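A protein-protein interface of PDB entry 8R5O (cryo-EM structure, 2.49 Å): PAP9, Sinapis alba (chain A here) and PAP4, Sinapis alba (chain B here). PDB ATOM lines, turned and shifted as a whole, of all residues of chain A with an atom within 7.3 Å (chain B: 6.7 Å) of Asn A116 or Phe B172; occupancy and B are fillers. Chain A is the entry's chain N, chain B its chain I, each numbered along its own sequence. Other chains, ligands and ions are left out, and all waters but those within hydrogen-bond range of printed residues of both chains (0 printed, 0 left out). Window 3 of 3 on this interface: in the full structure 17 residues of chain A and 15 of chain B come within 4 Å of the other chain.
OG of Ser B174 is in hydrogen-bond range of OG of Ser A171 (3.1 Å).
OH of Tyr A80 lies within hydrogen-bond range of NE2 of Gln A120 (3.2 Å). ND2 of Asn A123 is in hydrogen-bond range of O of Ala A208 (3.0 Å). N of Asn A207 is in hydrogen-bond range of O of Ser A171, 2.7 Å away. O of Asn A207 sits at hydrogen-bond distance from NE1 of Trp A225 (2.9 Å). The backbone carbonyl oxygen of Gly B173 lies within hydrogen-bond range of the guanidinium group of Arg B225, 3.4 Å away. O of Ser B174 sits at hydrogen-bond distance from N of Asn B195.
Among the printed residues, pairs that only touch across the chains: Asn A116 with Phe B172 (3.6 Å), Gln A120 with Phe B172 (3.95 Å), Asn A207 with Phe B172 (3.8 Å), Ala A208 with Phe B172 (3.9 Å), Trp A225 with Phe B172 (3.7 Å) and Trp A225 with Gly B173 (3.8 Å).
Asn A116 touches just one residue of chain B: Phe B172. Printed residues of chain B within 4 Å of Trp A225: Phe B172 (3.7 Å) and Gly B173 (3.8 Å). Printed residues of chain A within 4 Å of Gly B173: Trp A225. Of the printed residues of chain B, Gln A120 touches Phe B172 (3.95 Å). Of the printed residues of chain B, Ala A208 touches Phe B172 (3.9 Å). Of the printed residues of chain A, Ser B174 touches Ser A171.
Of the 23 printed residues of chain A, 6 touch a printed residue of chain B. Hydrophobic or aromatic side chains of chain A within 4 Å of the printed part of chain B: Ala A208 and Trp A225. Of the 14 printed residues of chain B, 3 touch a printed residue of chain A. Hydrophobic or aromatic side chains of chain B within 4 Å of the printed part of chain A: Phe B172. Along chain B the printed residues that touch a printed residue of chain A span positions 172 to 174. Among the printed residues, 7 pairs touch across the chains.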
ATOM      1  N   TYR A  80      19.395  -2.715  -8.944  1.00  0.00           N
ATOM      2  CA  TYR A  80      19.659  -3.707  -7.906  1.00  0.00           C
ATOM      3  C   TYR A  80      18.426  -4.555  -7.622  1.00  0.00           C
ATOM      4  O   TYR A  80      18.528  -5.776  -7.460  1.00  0.00           O
ATOM      5  CB  TYR A  80      20.137  -3.014  -6.629  1.00  0.00           C
ATOM      6  CG  TYR A  80      21.541  -2.464  -6.711  1.00  0.00           C
ATOM      7  CD1 TYR A  80      22.567  -3.208  -7.276  1.00  0.00           C
ATOM      8  CD2 TYR A  80      21.840  -1.197  -6.226  1.00  0.00           C
ATOM      9  CE1 TYR A  80      23.851  -2.710  -7.352  1.00  0.00           C
ATOM     10  CE2 TYR A  80      23.119  -0.690  -6.301  1.00  0.00           C
ATOM     11  CZ  TYR A  80      24.122  -1.450  -6.864  1.00  0.00           C
ATOM     12  OH  TYR A  80      25.400  -0.947  -6.938  1.00  0.00           O
ATOM     13  N   LEU A  84      17.959  -8.518  -8.652  1.00  0.00           N
ATOM     14  CA  LEU A  84      17.670  -9.424  -7.547  1.00  0.00           C
ATOM     15  C   LEU A  84      16.471 -10.313  -7.856  1.00  0.00           C
ATOM     16  O   LEU A  84      16.484 -11.511  -7.552  1.00  0.00           O
ATOM     17  CB  LEU A  84      17.430  -8.626  -6.266  1.00  0.00           C
ATOM     18  CG  LEU A  84      17.060  -9.412  -5.010  1.00  0.00           C
ATOM     19  CD1 LEU A  84      18.171 -10.375  -4.630  1.00  0.00           C
ATOM     20  CD2 LEU A  84      16.756  -8.462  -3.866  1.00  0.00           C
ATOM     21  N   GLN A  87      17.369 -13.276  -9.991  1.00  0.00           N
ATOM     22  CA  GLN A  87      18.145 -14.308  -9.316  1.00  0.00           C
ATOM     23  C   GLN A  87      17.327 -15.109  -8.311  1.00  0.00           C
ATOM     24  O   GLN A  87      17.793 -16.159  -7.854  1.00  0.00           O
ATOM     25  CB  GLN A  87      19.349 -13.680  -8.610  1.00  0.00           C
ATOM     26  CG  GLN A  87      20.334 -13.016  -9.555  1.00  0.00           C
ATOM     27  CD  GLN A  87      21.429 -12.269  -8.826  1.00  0.00           C
ATOM     28  OE1 GLN A  87      21.157 -11.412  -7.987  1.00  0.00           O
ATOM     29  NE2 GLN A  87      22.677 -12.593  -9.139  1.00  0.00           N
ATOM     30  N   SER A 105      22.376 -15.285   1.398  1.00  0.00           N
ATOM     31  CA  SER A 105      23.290 -15.125   0.277  1.00  0.00           C
ATOM     32  C   SER A 105      24.703 -14.767   0.716  1.00  0.00           C
ATOM     33  O   SER A 105      25.644 -14.967  -0.059  1.00  0.00           O
ATOM     34  CB  SER A 105      22.762 -14.059  -0.682  1.00  0.00           C
ATOM     35  OG  SER A 105      22.551 -12.832  -0.011  1.00  0.00           O
ATOM     36  N   MET A 111      30.246 -15.511  -0.387  1.00  0.00           N
ATOM     37  CA  MET A 111      29.039 -14.847  -0.860  1.00  0.00           C
ATOM     38  C   MET A 111      28.495 -15.502  -2.122  1.00  0.00           C
ATOM     39  O   MET A 111      29.236 -15.798  -3.063  1.00  0.00           O
ATOM     40  CB  MET A 111      29.324 -13.367  -1.118  1.00  0.00           C
ATOM     41  CG  MET A 111      29.986 -12.651   0.049  1.00  0.00           C
ATOM     42  SD  MET A 111      30.459 -10.953  -0.331  1.00  0.00           S
ATOM     43  CE  MET A 111      31.354 -10.507   1.155  1.00  0.00           C
ATOM     44  N   LEU A 112      27.186 -15.723  -2.132  1.00  0.00           N
ATOM     45  CA  LEU A 112      26.481 -16.266  -3.279  1.00  0.00           C
ATOM     46  C   LEU A 112      26.192 -15.156  -4.289  1.00  0.00           C
ATOM     47  O   LEU A 112      26.279 -13.972  -3.961  1.00  0.00           O
ATOM     48  CB  LEU A 112      25.194 -16.941  -2.816  1.00  0.00           C
ATOM     49  CG  LEU A 112      25.402 -18.165  -1.919  1.00  0.00           C
ATOM     50  CD1 LEU A 112      24.075 -18.778  -1.507  1.00  0.00           C
ATOM     51  CD2 LEU A 112      26.278 -19.196  -2.613  1.00  0.00           C
ATOM     52  N   PRO A 113      25.861 -15.513  -5.537  1.00  0.00           N
ATOM     53  CA  PRO A 113      25.675 -14.475  -6.567  1.00  0.00           C
ATOM     54  C   PRO A 113      24.621 -13.433  -6.226  1.00  0.00           C
ATOM     55  O   PRO A 113      24.732 -12.290  -6.685  1.00  0.00           O
ATOM     56  CB  PRO A 113      25.278 -15.286  -7.807  1.00  0.00           C
ATOM     57  CG  PRO A 113      25.913 -16.611  -7.595  1.00  0.00           C
ATOM     58  CD  PRO A 113      25.838 -16.868  -6.119  1.00  0.00           C
ATOM     59  N   ALA A 114      23.604 -13.786  -5.445  1.00  0.00           N
ATOM     60  CA  ALA A 114      22.533 -12.847  -5.136  1.00  0.00           C
ATOM     61  C   ALA A 114      22.908 -11.824  -4.072  1.00  0.00           C
ATOM     62  O   ALA A 114      22.169 -10.853  -3.893  1.00  0.00           O
ATOM     63  CB  ALA A 114      21.281 -13.605  -4.691  1.00  0.00           C
ATOM     64  N   PHE A 115      24.030 -12.009  -3.368  1.00  0.00           N
ATOM     65  CA  PHE A 115      24.325 -11.160  -2.216  1.00  0.00           C
ATOM     66  C   PHE A 115      24.522  -9.702  -2.614  1.00  0.00           C
ATOM     67  O   PHE A 115      24.018  -8.800  -1.938  1.00  0.00           O
ATOM     68  CB  PHE A 115      25.560 -11.670  -1.474  1.00  0.00           C
ATOM     69  CG  PHE A 115      25.979 -10.784  -0.334  1.00  0.00           C
ATOM     70  CD1 PHE A 115      25.322 -10.844   0.882  1.00  0.00           C
ATOM     71  CD2 PHE A 115      27.018  -9.881  -0.485  1.00  0.00           C
ATOM     72  CE1 PHE A 115      25.700 -10.028   1.929  1.00  0.00           C
ATOM     73  CE2 PHE A 115      27.398  -9.062   0.557  1.00  0.00           C
ATOM     74  CZ  PHE A 115      26.739  -9.135   1.766  1.00  0.00           C
ATOM     75  N   ASN A 116      25.262  -9.449  -3.696  1.00  0.00           N
ATOM     76  CA  ASN A 116      25.558  -8.069  -4.068  1.00  0.00           C
ATOM     77  C   ASN A 116      24.286  -7.298  -4.404  1.00  0.00           C
ATOM     78  O   ASN A 116      24.126  -6.146  -3.988  1.00  0.00           O
ATOM     79  CB  ASN A 116      26.537  -8.029  -5.239  1.00  0.00           C
ATOM     80  CG  ASN A 116      27.971  -8.246  -4.804  1.00  0.00           C
ATOM     81  OD1 ASN A 116      28.292  -8.153  -3.621  1.00  0.00           O
ATOM     82  ND2 ASN A 116      28.845  -8.528  -5.763  1.00  0.00           N
ATOM     83  N   ASN A 117      23.371  -7.916  -5.148  1.00  0.00           N
ATOM     84  CA  ASN A 117      22.107  -7.251  -5.448  1.00  0.00           C
ATOM     85  C   ASN A 117      21.232  -7.137  -4.206  1.00  0.00           C
ATOM     86  O   ASN A 117      20.612  -6.094  -3.974  1.00  0.00           O
ATOM     87  CB  ASN A 117      21.371  -7.997  -6.558  1.00  0.00           C
ATOM     88  CG  ASN A 117      22.092  -7.924  -7.886  1.00  0.00           C
ATOM     89  OD1 ASN A 117      22.710  -6.912  -8.216  1.00  0.00           O
ATOM     90  ND2 ASN A 117      22.021  -9.000  -8.658  1.00  0.00           N
ATOM     91  N   ALA A 118      21.171  -8.196  -3.397  1.00  0.00           N
ATOM     92  CA  ALA A 118      20.312  -8.185  -2.217  1.00  0.00           C
ATOM     93  C   ALA A 118      20.807  -7.186  -1.180  1.00  0.00           C
ATOM     94  O   ALA A 118      20.017  -6.417  -0.620  1.00  0.00           O
ATOM     95  CB  ALA A 118      20.229  -9.585  -1.614  1.00  0.00           C
ATOM     96  N   ALA A 119      22.111  -7.190  -0.903  1.00  0.00           N
ATOM     97  CA  ALA A 119      22.653  -6.289   0.108  1.00  0.00           C
ATOM     98  C   ALA A 119      22.550  -4.834  -0.331  1.00  0.00           C
ATOM     99  O   ALA A 119      22.203  -3.962   0.475  1.00  0.00           O
ATOM    100  CB  ALA A 119      24.100  -6.661   0.420  1.00  0.00           C
ATOM    101  N   GLN A 120      22.841  -4.547  -1.602  1.00  0.00           N
ATOM    102  CA  GLN A 120      22.741  -3.177  -2.093  1.00  0.00           C
ATOM    103  C   GLN A 120      21.300  -2.685  -2.085  1.00  0.00           C
ATOM    104  O   GLN A 120      21.042  -1.516  -1.780  1.00  0.00           O
ATOM    105  CB  GLN A 120      23.335  -3.068  -3.496  1.00  0.00           C
ATOM    106  CG  GLN A 120      24.853  -3.011  -3.533  1.00  0.00           C
ATOM    107  CD  GLN A 120      25.411  -1.732  -2.940  1.00  0.00           C
ATOM    108  OE1 GLN A 120      25.537  -1.601  -1.724  1.00  0.00           O
ATOM    109  NE2 GLN A 120      25.749  -0.780  -3.800  1.00  0.00           N
ATOM    110  N   ALA A 121      20.350  -3.558  -2.429  1.00  0.00           N
ATOM    111  CA  ALA A 121      18.944  -3.168  -2.388  1.00  0.00           C
ATOM    112  C   ALA A 121      18.516  -2.816  -0.970  1.00  0.00           C
ATOM    113  O   ALA A 121      17.786  -1.841  -0.759  1.00  0.00           O
ATOM    114  CB  ALA A 121      18.070  -4.285  -2.954  1.00  0.00           C
ATOM    115  N   TRP A 122      18.955  -3.600   0.015  1.00  0.00           N
ATOM    116  CA  TRP A 122      18.665  -3.269   1.406  1.00  0.00           C
ATOM    117  C   TRP A 122      19.387  -1.997   1.834  1.00  0.00           C
ATOM    118  O   TRP A 122      18.818  -1.168   2.552  1.00  0.00           O
ATOM    119  CB  TRP A 122      19.050  -4.434   2.318  1.00  0.00           C
ATOM    120  CG  TRP A 122      18.589  -4.252   3.729  1.00  0.00           C
ATOM    121  CD1 TRP A 122      17.418  -4.691   4.268  1.00  0.00           C
ATOM    122  CD2 TRP A 122      19.286  -3.572   4.780  1.00  0.00           C
ATOM    123  NE1 TRP A 122      17.341  -4.331   5.589  1.00  0.00           N
ATOM    124  CE2 TRP A 122      18.476  -3.644   5.928  1.00  0.00           C
ATOM    125  CE3 TRP A 122      20.516  -2.914   4.862  1.00  0.00           C
ATOM    126  CZ2 TRP A 122      18.855  -3.082   7.145  1.00  0.00           C
ATOM    127  CZ3 TRP A 122      20.890  -2.356   6.068  1.00  0.00           C
ATOM    128  CH2 TRP A 122      20.063  -2.444   7.194  1.00  0.00           C
ATOM    129  N   ASN A 123      20.644  -1.831   1.408  1.00  0.00           N
ATOM    130  CA  ASN A 123      21.427  -0.676   1.832  1.00  0.00           C
ATOM    131  C   ASN A 123      20.798   0.630   1.368  1.00  0.00           C
ATOM    132  O   ASN A 123      20.735   1.602   2.130  1.00  0.00           O
ATOM    133  CB  ASN A 123      22.858  -0.786   1.305  1.00  0.00           C
ATOM    134  CG  ASN A 123      23.664  -1.850   2.014  1.00  0.00           C
ATOM    135  OD1 ASN A 123      23.354  -2.233   3.139  1.00  0.00           O
ATOM    136  ND2 ASN A 123      24.708  -2.333   1.356  1.00  0.00           N
ATOM    137  N   SER A 171      34.580   2.130  -2.846  1.00  0.00           N
ATOM    138  CA  SER A 171      33.142   2.104  -2.628  1.00  0.00           C
ATOM    139  C   SER A 171      32.822   1.409  -1.312  1.00  0.00           C
ATOM    140  O   SER A 171      33.416   0.382  -0.976  1.00  0.00           O
ATOM    141  CB  SER A 171      32.442   1.384  -3.781  1.00  0.00           C
ATOM    142  OG  SER A 171      32.744   1.988  -5.024  1.00  0.00           O
ATOM    143  N   PRO A 206      33.094  -2.356   2.958  1.00  0.00           N
ATOM    144  CA  PRO A 206      33.359  -2.149   1.532  1.00  0.00           C
ATOM    145  C   PRO A 206      32.232  -2.652   0.645  1.00  0.00           C
ATOM    146  O   PRO A 206      31.552  -3.636   0.944  1.00  0.00           O
ATOM    147  CB  PRO A 206      34.635  -2.969   1.307  1.00  0.00           C
ATOM    148  CG  PRO A 206      34.501  -4.098   2.262  1.00  0.00           C
ATOM    149  CD  PRO A 206      33.777  -3.556   3.474  1.00  0.00           C
ATOM    150  N   ASN A 207      32.044  -1.942  -0.467  1.00  0.00           N
ATOM    151  CA  ASN A 207      31.105  -2.322  -1.518  1.00  0.00           C
ATOM    152  C   ASN A 207      29.678  -2.485  -1.004  1.00  0.00           C
ATOM    153  O   ASN A 207      29.010  -1.495  -0.693  1.00  0.00           O
ATOM    154  CB  ASN A 207      31.572  -3.607  -2.205  1.00  0.00           C
ATOM    155  CG  ASN A 207      32.882  -3.426  -2.949  1.00  0.00           C
ATOM    156  OD1 ASN A 207      33.257  -2.309  -3.305  1.00  0.00           O
ATOM    157  ND2 ASN A 207      33.582  -4.524  -3.192  1.00  0.00           N
ATOM    158  N   ALA A 208      29.199  -3.725  -0.925  1.00  0.00           N
ATOM    159  CA  ALA A 208      27.816  -4.008  -0.567  1.00  0.00           C
ATOM    160  C   ALA A 208      27.648  -4.547   0.846  1.00  0.00           C
ATOM    161  O   ALA A 208      26.513  -4.784   1.268  1.00  0.00           O
ATOM    162  CB  ALA A 208      27.205  -4.997  -1.566  1.00  0.00           C
ATOM    163  N   VAL A 209      28.736  -4.743   1.589  1.00  0.00           N
ATOM    164  CA  VAL A 209      28.645  -5.339   2.915  1.00  0.00           C
ATOM    165  C   VAL A 209      27.925  -4.389   3.865  1.00  0.00           C
ATOM    166  O   VAL A 209      28.080  -3.165   3.787  1.00  0.00           O
ATOM    167  CB  VAL A 209      30.050  -5.697   3.427  1.00  0.00           C
ATOM    168  CG1 VAL A 209      29.983  -6.346   4.801  1.00  0.00           C
ATOM    169  CG2 VAL A 209      30.753  -6.614   2.438  1.00  0.00           C
ATOM    170  N   TRP A 225      29.714   5.373  -1.953  1.00  0.00           N
ATOM    171  CA  TRP A 225      29.934   5.126  -3.369  1.00  0.00           C
ATOM    172  C   TRP A 225      29.963   6.460  -4.101  1.00  0.00           C
ATOM    173  O   TRP A 225      29.213   7.382  -3.770  1.00  0.00           O
ATOM    174  CB  TRP A 225      28.834   4.232  -3.945  1.00  0.00           C
ATOM    175  CG  TRP A 225      28.922   2.783  -3.555  1.00  0.00           C
ATOM    176  CD1 TRP A 225      28.870   2.267  -2.295  1.00  0.00           C
ATOM    177  CD2 TRP A 225      29.038   1.664  -4.441  1.00  0.00           C
ATOM    178  NE1 TRP A 225      28.964   0.900  -2.337  1.00  0.00           N
ATOM    179  CE2 TRP A 225      29.068   0.502  -3.644  1.00  0.00           C
ATOM    180  CE3 TRP A 225      29.131   1.531  -5.828  1.00  0.00           C
ATOM    181  CZ2 TRP A 225      29.185  -0.773  -4.189  1.00  0.00           C
ATOM    182  CZ3 TRP A 225      29.246   0.265  -6.367  1.00  0.00           C
ATOM    183  CH2 TRP A 225      29.273  -0.871  -5.550  1.00  0.00           C
ATOM    184  N   ALA B 167      35.196  -8.872 -18.138  1.00  0.00           N
ATOM    185  CA  ALA B 167      35.916  -8.556 -16.909  1.00  0.00           C
ATOM    186  C   ALA B 167      35.578  -7.153 -16.422  1.00  0.00           C
ATOM    187  O   ALA B 167      35.437  -6.922 -15.216  1.00  0.00           O
ATOM    188  CB  ALA B 167      37.421  -8.701 -17.126  1.00  0.00           C
ATOM    189  N   ALA B 168      35.446  -6.204 -17.347  1.00  0.00           N
ATOM    190  CA  ALA B 168      35.131  -4.831 -16.973  1.00  0.00           C
ATOM    191  C   ALA B 168      33.677  -4.663 -16.556  1.00  0.00           C
ATOM    192  O   ALA B 168      33.381  -3.836 -15.687  1.00  0.00           O
ATOM    193  CB  ALA B 168      35.465  -3.889 -18.128  1.00  0.00           C
ATOM    194  N   LEU B 169      32.761  -5.423 -17.157  1.00  0.00           N
ATOM    195  CA  LEU B 169      31.353  -5.326 -16.791  1.00  0.00           C
ATOM    196  C   LEU B 169      31.052  -6.001 -15.460  1.00  0.00           C
ATOM    197  O   LEU B 169      30.098  -5.610 -14.778  1.00  0.00           O
ATOM    198  CB  LEU B 169      30.478  -5.930 -17.889  1.00  0.00           C
ATOM    199  CG  LEU B 169      30.235  -5.090 -19.143  1.00  0.00           C
ATOM    200  CD1 LEU B 169      29.447  -5.885 -20.167  1.00  0.00           C
ATOM    201  CD2 LEU B 169      29.507  -3.807 -18.786  1.00  0.00           C
ATOM    202  N   THR B 170      31.837  -7.002 -15.071  1.00  0.00           N
ATOM    203  CA  THR B 170      31.559  -7.784 -13.875  1.00  0.00           C
ATOM    204  C   THR B 170      32.403  -7.378 -12.674  1.00  0.00           C
ATOM    205  O   THR B 170      32.212  -7.933 -11.589  1.00  0.00           O
ATOM    206  CB  THR B 170      31.759  -9.276 -14.158  1.00  0.00           C
ATOM    207  OG1 THR B 170      33.087  -9.502 -14.642  1.00  0.00           O
ATOM    208  CG2 THR B 170      30.759  -9.758 -15.194  1.00  0.00           C
ATOM    209  N   GLN B 171      33.329  -6.437 -12.835  1.00  0.00           N
ATOM    210  CA  GLN B 171      34.076  -5.915 -11.694  1.00  0.00           C
ATOM    211  C   GLN B 171      33.136  -5.080 -10.835  1.00  0.00           C
ATOM    212  O   GLN B 171      32.679  -4.013 -11.256  1.00  0.00           O
ATOM    213  CB  GLN B 171      35.270  -5.093 -12.166  1.00  0.00           C
ATOM    214  CG  GLN B 171      36.006  -4.361 -11.053  1.00  0.00           C
ATOM    215  CD  GLN B 171      36.592  -5.297 -10.013  1.00  0.00           C
ATOM    216  OE1 GLN B 171      37.124  -6.356 -10.344  1.00  0.00           O
ATOM    217  NE2 GLN B 171      36.495  -4.912  -8.749  1.00  0.00           N
ATOM    218  N   PHE B 172      32.838  -5.565  -9.633  1.00  0.00           N
ATOM    219  CA  PHE B 172      31.876  -4.918  -8.753  1.00  0.00           C
ATOM    220  C   PHE B 172      32.574  -3.854  -7.918  1.00  0.00           C
ATOM    221  O   PHE B 172      33.595  -4.128  -7.278  1.00  0.00           O
ATOM    222  CB  PHE B 172      31.200  -5.951  -7.851  1.00  0.00           C
ATOM    223  CG  PHE B 172      30.078  -5.392  -7.024  1.00  0.00           C
ATOM    224  CD1 PHE B 172      28.877  -5.039  -7.614  1.00  0.00           C
ATOM    225  CD2 PHE B 172      30.220  -5.234  -5.657  1.00  0.00           C
ATOM    226  CE1 PHE B 172      27.843  -4.529  -6.858  1.00  0.00           C
ATOM    227  CE2 PHE B 172      29.187  -4.726  -4.896  1.00  0.00           C
ATOM    228  CZ  PHE B 172      27.998  -4.374  -5.498  1.00  0.00           C
ATOM    229  N   GLY B 173      32.023  -2.646  -7.927  1.00  0.00           N
ATOM    230  CA  GLY B 173      32.627  -1.546  -7.207  1.00  0.00           C
ATOM    231  C   GLY B 173      33.814  -0.960  -7.952  1.00  0.00           C
ATOM    232  O   GLY B 173      33.994  -1.145  -9.159  1.00  0.00           O
ATOM    233  N   SER B 174      34.637  -0.233  -7.204  1.00  0.00           N
ATOM    234  CA  SER B 174      35.828   0.379  -7.774  1.00  0.00           C
ATOM    235  C   SER B 174      36.879  -0.681  -8.079  1.00  0.00           C
ATOM    236  O   SER B 174      37.021  -1.663  -7.348  1.00  0.00           O
ATOM    237  CB  SER B 174      36.398   1.418  -6.812  1.00  0.00           C
ATOM    238  OG  SER B 174      35.446   2.423  -6.526  1.00  0.00           O
ATOM    239  N   GLY B 175      37.617  -0.479  -9.163  1.00  0.00           N
ATOM    240  CA  GLY B 175      38.653  -1.425  -9.520  1.00  0.00           C
ATOM    241  C   GLY B 175      39.294  -1.074 -10.847  1.00  0.00           C
ATOM    242  O   GLY B 175      39.119   0.023 -11.378  1.00  0.00           O
ATOM    243  N   LYS B 192      41.093  -8.665 -13.592  1.00  0.00           N
ATOM    244  CA  LYS B 192      40.412  -7.549 -12.956  1.00  0.00           C
ATOM    245  C   LYS B 192      40.745  -7.535 -11.471  1.00  0.00           C
ATOM    246  O   LYS B 192      40.804  -8.586 -10.827  1.00  0.00           O
ATOM    247  CB  LYS B 192      38.890  -7.617 -13.166  1.00  0.00           C
ATOM    248  CG  LYS B 192      38.199  -8.815 -12.535  1.00  0.00           C
ATOM    249  CD  LYS B 192      36.690  -8.720 -12.706  1.00  0.00           C
ATOM    250  CE  LYS B 192      35.964  -9.802 -11.927  1.00  0.00           C
ATOM    251  NZ  LYS B 192      36.319 -11.169 -12.390  1.00  0.00           N
ATOM    252  N   THR B 193      40.989  -6.340 -10.939  1.00  0.00           N
ATOM    253  CA  THR B 193      41.343  -6.157  -9.540  1.00  0.00           C
ATOM    254  C   THR B 193      40.430  -5.107  -8.927  1.00  0.00           C
ATOM    255  O   THR B 193      39.806  -4.312  -9.631  1.00  0.00           O
ATOM    256  CB  THR B 193      42.814  -5.739  -9.370  1.00  0.00           C
ATOM    257  OG1 THR B 193      43.035  -4.474 -10.002  1.00  0.00           O
ATOM    258  CG2 THR B 193      43.742  -6.776  -9.984  1.00  0.00           C
ATOM    259  N   SER B 194      40.350  -5.114  -7.600  1.00  0.00           N
ATOM    260  CA  SER B 194      39.484  -4.210  -6.859  1.00  0.00           C
ATOM    261  C   SER B 194      40.304  -3.111  -6.197  1.00  0.00           C
ATOM    262  O   SER B 194      41.423  -3.351  -5.733  1.00  0.00           O
ATOM    263  CB  SER B 194      38.680  -4.967  -5.798  1.00  0.00           C
ATOM    264  OG  SER B 194      39.532  -5.540  -4.824  1.00  0.00           O
ATOM    265  N   ASN B 195      39.735  -1.905  -6.165  1.00  0.00           N
ATOM    266  CA  ASN B 195      40.323  -0.729  -5.512  1.00  0.00           C
ATOM    267  C   ASN B 195      41.651  -0.406  -6.190  1.00  0.00           C
ATOM    268  O   ASN B 195      41.648  -0.130  -7.401  1.00  0.00           O
ATOM    269  CB  ASN B 195      40.387  -0.979  -4.003  1.00  0.00           C
ATOM    270  CG  ASN B 195      39.018  -0.952  -3.352  1.00  0.00           C
ATOM    271  OD1 ASN B 195      37.999  -0.829  -4.028  1.00  0.00           O
ATOM    272  ND2 ASN B 195      38.991  -1.076  -2.032  1.00  0.00           N
ATOM    273  N   ARG B 225      28.260   1.962 -17.699  1.00  0.00           N
ATOM    274  CA  ARG B 225      29.647   1.518 -17.785  1.00  0.00           C
ATOM    275  C   ARG B 225      29.912   0.775 -19.085  1.00  0.00           C
ATOM    276  O   ARG B 225      31.018   0.856 -19.629  1.00  0.00           O
ATOM    277  CB  ARG B 225      30.003   0.636 -16.587  1.00  0.00           C
ATOM    278  CG  ARG B 225      31.486   0.318 -16.500  1.00  0.00           C
ATOM    279  CD  ARG B 225      31.782  -0.829 -15.556  1.00  0.00           C
ATOM    280  NE  ARG B 225      31.731  -0.433 -14.155  1.00  0.00           N
ATOM    281  CZ  ARG B 225      32.134  -1.198 -13.151  1.00  0.00           C
ATOM    282  NH1 ARG B 225      32.625  -2.408 -13.358  1.00  0.00           N
ATOM    283  NH2 ARG B 225      32.049  -0.734 -11.908  1.00  0.00           N
